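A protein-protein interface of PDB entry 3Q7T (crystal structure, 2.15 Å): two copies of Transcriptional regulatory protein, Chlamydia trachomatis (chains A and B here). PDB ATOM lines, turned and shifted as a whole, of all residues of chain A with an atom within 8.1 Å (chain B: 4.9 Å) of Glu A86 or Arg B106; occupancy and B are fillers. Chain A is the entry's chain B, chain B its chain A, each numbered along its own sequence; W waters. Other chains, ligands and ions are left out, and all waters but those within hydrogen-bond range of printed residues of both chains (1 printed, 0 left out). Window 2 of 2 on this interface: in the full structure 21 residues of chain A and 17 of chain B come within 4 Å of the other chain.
Among the printed residues, pairs that only touch across the chains: Phe A83 with Ile B107 (3.5 Å), Glu A85 with Ile B107 (3.8 Å), Val A89 with Arg B106 (3.9 Å), Val A89 with Ile B107 (3.6 Å), Val A89 with Ser B110 (3.9 Å), Leu A92 with Ile B107 (3.6 Å) and Leu A92 with Ser B110 (3.6 Å).
Hydrophobic or aromatic side chains of chain A that line the printed part of chain B: Phe A83, Val A89 and Leu A92.
Along chain A the printed residues that touch a printed residue of chain B span positions 83 to 93.
Of the 8 printed residues of chain B, 4 touch a printed residue of chain A.
Printed residues of chain B that touch a printed residue of chain A: Thr B104, Arg B106, Ile B107 and Ser B110.
Among the printed residues, 11 pairs touch across the chains.
Among the printed residues, Asp or Glu carboxylates within 4 Å of a Lys or Arg side-chain nitrogen of the other chain: Glu A85 with Arg B106 (3.1 Å) and Glu A86 with Arg B106 (2.9 Å).
No position is printed for both chains.
The backbone NH of Ile B107 lies within hydrogen-bond range of the side-chain hydroxyl of Thr B104, at 3.1 Å.
The backbone carbonyl oxygen (O) of Arg B106 sits at hydrogen-bond distance from the side-chain hydroxyl (OG) of Ser B110, at 2.9 Å.
Of the printed residues of chain B, Phe A83 touches Ile B107 (3.5 Å).
Printed residues of chain B within 4 Å of Glu A86: Arg B106 (2.9 Å).
Of the printed residues of chain B, Leu A92 touches Ile B107 (3.6 Å) and Ser B110 (3.6 Å).
Arg A94 touches none of the printed residues of chain B.
Arg B106 touches just these residues of chain A: Glu A85 (3.1 Å), Glu A86 (2.9 Å) and Val A89 (3.9 Å).
Leu B108 touches none of the printed residues of chain A.
The nearest printed residue of chain B that does not touch Glu A86 is Ile B107 (6.1 Å).
The nearest residue of chain A that does not touch Arg B106 is Leu A92 (5.5 Å).
The nearest printed residue of chain B that does not touch Asp A93 is Arg B106 (5.8 Å).
Water W1 bridges the backbone carbonyl oxygen (O) of Ser B110 (3.0 Å) and the backbone carbonyl oxygen (O) of Leu A92 (3.0 Å).
The side-chain hydroxyl (OG1) of Thr B104 is in hydrogen-bond range of the side-chain carboxylate (OE2) of Glu A85 (2.8 Å).
The side-chain carboxylate (OD1) of Asp A93 is in hydrogen-bond range of the side-chain hydroxyl (OG) of Ser B110, 3.0 Å away.
OE2 of Glu A86 lies within salt-bridge range of NH1 of Arg B106 (2.9 Å).
The side-chain carboxylate (OE2) of Glu A85 lies within salt-bridge range of the guanidinium group (NH1) of Arg B106 (3.1 Å).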
ATOM      1  N   TYR A  58      35.657  29.133  -0.016  1.00  0.00           N
ATOM      2  CA  TYR A  58      34.323  29.132  -0.607  1.00  0.00           C
ATOM      3  C   TYR A  58      33.655  30.499  -0.573  1.00  0.00           C
ATOM      4  O   TYR A  58      32.957  30.865  -1.511  1.00  0.00           O
ATOM      5  CB  TYR A  58      33.424  28.077   0.069  1.00  0.00           C
ATOM      6  CG  TYR A  58      31.999  28.023  -0.474  1.00  0.00           C
ATOM      7  CD1 TYR A  58      31.716  27.448  -1.715  1.00  0.00           C
ATOM      8  CD2 TYR A  58      30.930  28.527   0.268  1.00  0.00           C
ATOM      9  CE1 TYR A  58      30.396  27.399  -2.212  1.00  0.00           C
ATOM     10  CE2 TYR A  58      29.635  28.485  -0.213  1.00  0.00           C
ATOM     11  CZ  TYR A  58      29.371  27.926  -1.451  1.00  0.00           C
ATOM     12  OH  TYR A  58      28.070  27.899  -1.905  1.00  0.00           O
ATOM     13  N   PHE A  83      30.360  20.995   6.033  1.00  0.00           N
ATOM     14  CA  PHE A  83      29.686  20.150   5.073  1.00  0.00           C
ATOM     15  C   PHE A  83      28.238  20.602   4.882  1.00  0.00           C
ATOM     16  O   PHE A  83      27.518  20.860   5.844  1.00  0.00           O
ATOM     17  CB  PHE A  83      29.693  18.697   5.519  1.00  0.00           C
ATOM     18  CG  PHE A  83      28.902  17.788   4.610  1.00  0.00           C
ATOM     19  CD1 PHE A  83      29.457  17.304   3.436  1.00  0.00           C
ATOM     20  CD2 PHE A  83      27.601  17.423   4.931  1.00  0.00           C
ATOM     21  CE1 PHE A  83      28.732  16.459   2.598  1.00  0.00           C
ATOM     22  CE2 PHE A  83      26.874  16.585   4.099  1.00  0.00           C
ATOM     23  CZ  PHE A  83      27.445  16.094   2.931  1.00  0.00           C
ATOM     24  N   ASP A  84      27.836  20.708   3.625  1.00  0.00           N
ATOM     25  CA  ASP A  84      26.445  20.899   3.251  1.00  0.00           C
ATOM     26  C   ASP A  84      26.314  20.149   1.933  1.00  0.00           C
ATOM     27  O   ASP A  84      27.164  20.313   1.043  1.00  0.00           O
ATOM     28  CB  ASP A  84      26.134  22.384   3.088  1.00  0.00           C
ATOM     29  CG  ASP A  84      24.747  22.637   2.507  1.00  0.00           C
ATOM     30  OD1 ASP A  84      23.756  22.486   3.247  1.00  0.00           O
ATOM     31  OD2 ASP A  84      24.644  23.018   1.317  1.00  0.00           O
ATOM     32  N   GLU A  85      25.305  19.280   1.839  1.00  0.00           N
ATOM     33  CA  GLU A  85      25.183  18.373   0.703  1.00  0.00           C
ATOM     34  C   GLU A  85      25.004  19.085  -0.632  1.00  0.00           C
ATOM     35  O   GLU A  85      25.603  18.692  -1.635  1.00  0.00           O
ATOM     36  CB  GLU A  85      24.033  17.363   0.887  1.00  0.00           C
ATOM     37  CG  GLU A  85      23.976  16.379  -0.315  1.00  0.00           C
ATOM     38  CD  GLU A  85      22.727  15.521  -0.377  1.00  0.00           C
ATOM     39  OE1 GLU A  85      21.837  15.698   0.491  1.00  0.00           O
ATOM     40  OE2 GLU A  85      22.637  14.675  -1.312  1.00  0.00           O
ATOM     41  N   GLU A  86      24.166  20.117  -0.653  1.00  0.00           N
ATOM     42  CA  GLU A  86      23.837  20.794  -1.902  1.00  0.00           C
ATOM     43  C   GLU A  86      25.055  21.528  -2.388  1.00  0.00           C
ATOM     44  O   GLU A  86      25.365  21.536  -3.586  1.00  0.00           O
ATOM     45  CB  GLU A  86      22.688  21.800  -1.716  1.00  0.00           C
ATOM     46  CG  GLU A  86      21.293  21.200  -1.799  1.00  0.00           C
ATOM     47  CD  GLU A  86      21.159  20.084  -2.834  1.00  0.00           C
ATOM     48  OE1 GLU A  86      21.334  20.334  -4.053  1.00  0.00           O
ATOM     49  OE2 GLU A  86      20.870  18.940  -2.417  1.00  0.00           O
ATOM     50  N   THR A  87      25.729  22.174  -1.444  1.00  0.00           N
ATOM     51  CA  THR A  87      26.960  22.890  -1.735  1.00  0.00           C
ATOM     52  C   THR A  87      28.012  21.947  -2.284  1.00  0.00           C
ATOM     53  O   THR A  87      28.641  22.260  -3.283  1.00  0.00           O
ATOM     54  CB  THR A  87      27.521  23.579  -0.490  1.00  0.00           C
ATOM     55  OG1 THR A  87      26.504  24.407   0.071  1.00  0.00           O
ATOM     56  CG2 THR A  87      28.718  24.434  -0.857  1.00  0.00           C
ATOM     57  N   SER A  88      28.203  20.794  -1.650  1.00  0.00           N
ATOM     58  CA  SER A  88      29.182  19.815  -2.168  1.00  0.00           C
ATOM     59  C   SER A  88      28.817  19.314  -3.570  1.00  0.00           C
ATOM     60  O   SER A  88      29.677  19.256  -4.459  1.00  0.00           O
ATOM     61  CB  SER A  88      29.329  18.601  -1.246  1.00  0.00           C
ATOM     62  OG  SER A  88      29.684  19.007   0.056  1.00  0.00           O
ATOM     63  N   VAL A  89      27.551  18.949  -3.774  1.00  0.00           N
ATOM     64  CA  VAL A  89      27.131  18.511  -5.111  1.00  0.00           C
ATOM     65  C   VAL A  89      27.334  19.629  -6.140  1.00  0.00           C
ATOM     66  O   VAL A  89      27.830  19.399  -7.226  1.00  0.00           O
ATOM     67  CB  VAL A  89      25.674  17.986  -5.151  1.00  0.00           C
ATOM     68  CG1 VAL A  89      25.249  17.701  -6.606  1.00  0.00           C
ATOM     69  CG2 VAL A  89      25.548  16.730  -4.318  1.00  0.00           C
ATOM     70  N   ASP A  90      26.967  20.845  -5.773  1.00  0.00           N
ATOM     71  CA  ASP A  90      27.140  21.999  -6.644  1.00  0.00           C
ATOM     72  C   ASP A  90      28.610  22.210  -7.039  1.00  0.00           C
ATOM     73  O   ASP A  90      28.922  22.441  -8.199  1.00  0.00           O
ATOM     74  CB  ASP A  90      26.580  23.243  -5.952  1.00  0.00           C
ATOM     75  CG  ASP A  90      26.665  24.489  -6.818  1.00  0.00           C
ATOM     76  OD1 ASP A  90      26.114  24.471  -7.944  1.00  0.00           O
ATOM     77  OD2 ASP A  90      27.277  25.489  -6.371  1.00  0.00           O
ATOM     78  N   LEU A  91      29.527  22.109  -6.084  1.00  0.00           N
ATOM     79  CA  LEU A  91      30.934  22.349  -6.406  1.00  0.00           C
ATOM     80  C   LEU A  91      31.471  21.310  -7.382  1.00  0.00           C
ATOM     81  O   LEU A  91      32.146  21.652  -8.353  1.00  0.00           O
ATOM     82  CB  LEU A  91      31.802  22.384  -5.133  1.00  0.00           C
ATOM     83  CG  LEU A  91      31.578  23.593  -4.220  1.00  0.00           C
ATOM     84  CD1 LEU A  91      32.276  23.398  -2.860  1.00  0.00           C
ATOM     85  CD2 LEU A  91      32.045  24.885  -4.913  1.00  0.00           C
ATOM     86  N   LEU A  92      31.179  20.038  -7.110  1.00  0.00           N
ATOM     87  CA  LEU A  92      31.636  18.936  -7.948  1.00  0.00           C
ATOM     88  C   LEU A  92      31.091  19.004  -9.389  1.00  0.00           C
ATOM     89  O   LEU A  92      31.825  18.750 -10.345  1.00  0.00           O
ATOM     90  CB  LEU A  92      31.274  17.586  -7.302  1.00  0.00           C
ATOM     91  CG  LEU A  92      31.936  17.246  -5.964  1.00  0.00           C
ATOM     92  CD1 LEU A  92      31.218  16.088  -5.251  1.00  0.00           C
ATOM     93  CD2 LEU A  92      33.441  16.967  -6.139  1.00  0.00           C
ATOM     94  N   ASP A  93      29.804  19.311  -9.527  1.00  0.00           N
ATOM     95  CA  ASP A  93      29.179  19.568 -10.838  1.00  0.00           C
ATOM     96  C   ASP A  93      29.786  20.759 -11.602  1.00  0.00           C
ATOM     97  O   ASP A  93      29.870  20.744 -12.821  1.00  0.00           O
ATOM     98  CB  ASP A  93      27.663  19.762 -10.671  1.00  0.00           C
ATOM     99  CG  ASP A  93      26.938  18.449 -10.319  1.00  0.00           C
ATOM    100  OD1 ASP A  93      27.577  17.376 -10.337  1.00  0.00           O
ATOM    101  OD2 ASP A  93      25.728  18.476 -10.039  1.00  0.00           O
ATOM    102  N   ARG A  94      30.225  21.787 -10.885  1.00  0.00           N
ATOM    103  CA  ARG A  94      30.929  22.896 -11.522  1.00  0.00           C
ATOM    104  C   ARG A  94      32.372  22.533 -11.879  1.00  0.00           C
ATOM    105  O   ARG A  94      33.103  23.355 -12.411  1.00  0.00           O
ATOM    106  CB  ARG A  94      30.900  24.127 -10.602  1.00  0.00           C
ATOM    107  CG  ARG A  94      29.484  24.641 -10.344  1.00  0.00           C
ATOM    108  CD  ARG A  94      29.397  25.516  -9.096  1.00  0.00           C
ATOM    109  NE  ARG A  94      30.175  26.748  -9.178  1.00  0.00           N
ATOM    110  CZ  ARG A  94      30.275  27.622  -8.170  1.00  0.00           C
ATOM    111  NH1 ARG A  94      29.641  27.394  -7.023  1.00  0.00           N
ATOM    112  NH2 ARG A  94      30.999  28.728  -8.301  1.00  0.00           N
ATOM    113  N   LEU B  31      22.403   6.304 -10.317  1.00  0.00           N
ATOM    114  CA  LEU B  31      22.601   7.697 -10.705  1.00  0.00           C
ATOM    115  C   LEU B  31      23.590   7.865 -11.859  1.00  0.00           C
ATOM    116  O   LEU B  31      23.487   8.798 -12.601  1.00  0.00           O
ATOM    117  CB  LEU B  31      23.051   8.540  -9.499  1.00  0.00           C
ATOM    118  CG  LEU B  31      22.006   9.389  -8.751  1.00  0.00           C
ATOM    119  CD1 LEU B  31      20.663   8.719  -8.641  1.00  0.00           C
ATOM    120  CD2 LEU B  31      22.485   9.828  -7.374  1.00  0.00           C
ATOM    121  N   THR B 104      26.596  11.215   0.190  1.00  0.00           N
ATOM    122  CA  THR B 104      25.329  10.797  -0.388  1.00  0.00           C
ATOM    123  C   THR B 104      25.572  10.214  -1.774  1.00  0.00           C
ATOM    124  O   THR B 104      26.642  10.420  -2.360  1.00  0.00           O
ATOM    125  CB  THR B 104      24.340  11.974  -0.542  1.00  0.00           C
ATOM    126  OG1 THR B 104      24.846  12.900  -1.521  1.00  0.00           O
ATOM    127  CG2 THR B 104      24.093  12.672   0.802  1.00  0.00           C
ATOM    128  N   PRO B 105      24.578   9.482  -2.298  1.00  0.00           N
ATOM    129  CA  PRO B 105      24.676   8.956  -3.661  1.00  0.00           C
ATOM    130  C   PRO B 105      24.981  10.064  -4.677  1.00  0.00           C
ATOM    131  O   PRO B 105      25.857   9.863  -5.503  1.00  0.00           O
ATOM    132  CB  PRO B 105      23.291   8.326  -3.894  1.00  0.00           C
ATOM    133  CG  PRO B 105      22.826   7.946  -2.517  1.00  0.00           C
ATOM    134  CD  PRO B 105      23.383   8.980  -1.577  1.00  0.00           C
ATOM    135  N   ARG B 106      24.323  11.222  -4.588  1.00  0.00           N
ATOM    136  CA  ARG B 106      24.624  12.339  -5.497  1.00  0.00           C
ATOM    137  C   ARG B 106      26.060  12.872  -5.378  1.00  0.00           C
ATOM    138  O   ARG B 106      26.702  13.193  -6.374  1.00  0.00           O
ATOM    139  CB  ARG B 106      23.609  13.474  -5.309  1.00  0.00           C
ATOM    140  CG  ARG B 106      22.202  13.105  -5.784  1.00  0.00           C
ATOM    141  CD  ARG B 106      21.124  14.049  -5.257  1.00  0.00           C
ATOM    142  NE  ARG B 106      21.317  15.434  -5.677  1.00  0.00           N
ATOM    143  CZ  ARG B 106      21.337  16.481  -4.849  1.00  0.00           C
ATOM    144  NH1 ARG B 106      21.196  16.308  -3.538  1.00  0.00           N
ATOM    145  NH2 ARG B 106      21.501  17.708  -5.331  1.00  0.00           N
ATOM    146  N   ILE B 107      26.557  12.996  -4.158  1.00  0.00           N
ATOM    147  CA  ILE B 107      27.935  13.426  -3.962  1.00  0.00           C
ATOM    148  C   ILE B 107      28.883  12.402  -4.590  1.00  0.00           C
ATOM    149  O   ILE B 107      29.795  12.770  -5.288  1.00  0.00           O
ATOM    150  CB  ILE B 107      28.264  13.632  -2.456  1.00  0.00           C
ATOM    151  CG1 ILE B 107      27.628  14.931  -1.949  1.00  0.00           C
ATOM    152  CG2 ILE B 107      29.780  13.627  -2.232  1.00  0.00           C
ATOM    153  CD1 ILE B 107      27.574  15.072  -0.438  1.00  0.00           C
ATOM    154  N   LEU B 108      28.649  11.115  -4.353  1.00  0.00           N
ATOM    155  CA  LEU B 108      29.555  10.086  -4.838  1.00  0.00           C
ATOM    156  C   LEU B 108      29.518   9.979  -6.376  1.00  0.00           C
ATOM    157  O   LEU B 108      30.559   9.882  -7.016  1.00  0.00           O
ATOM    158  CB  LEU B 108      29.273   8.736  -4.184  1.00  0.00           C
ATOM    159  CG  LEU B 108      30.310   7.687  -4.617  1.00  0.00           C
ATOM    160  CD1 LEU B 108      31.748   8.165  -4.333  1.00  0.00           C
ATOM    161  CD2 LEU B 108      30.057   6.346  -3.960  1.00  0.00           C
ATOM    162  N   LYS B 109      28.323  10.040  -6.962  1.00  0.00           N
ATOM    163  CA  LYS B 109      28.197  10.120  -8.420  1.00  0.00           C
ATOM    164  C   LYS B 109      28.934  11.316  -9.026  1.00  0.00           C
ATOM    165  O   LYS B 109      29.581  11.188 -10.054  1.00  0.00           O
ATOM    166  CB  LYS B 109      26.729  10.181  -8.827  1.00  0.00           C
ATOM    167  CG  LYS B 109      26.539  10.490 -10.294  1.00  0.00           C
ATOM    168  CD  LYS B 109      25.638  11.675 -10.483  1.00  0.00           C
ATOM    169  CE  LYS B 109      25.071  11.697 -11.904  1.00  0.00           C
ATOM    170  NZ  LYS B 109      24.049  12.750 -12.015  1.00  0.00           N
ATOM    171  N   SER B 110      28.831  12.487  -8.398  1.00  0.00           N
ATOM    172  CA  SER B 110      29.493  13.674  -8.929  1.00  0.00           C
ATOM    173  C   SER B 110      31.030  13.585  -8.815  1.00  0.00           C
ATOM    174  O   SER B 110      31.755  14.054  -9.685  1.00  0.00           O
ATOM    175  CB  SER B 110      28.978  14.939  -8.242  1.00  0.00           C
ATOM    176  OG  SER B 110      27.574  15.070  -8.384  1.00  0.00           O
HETATM  177  O   HOH W   1      30.719  16.200 -11.458  1.00  0.00           O
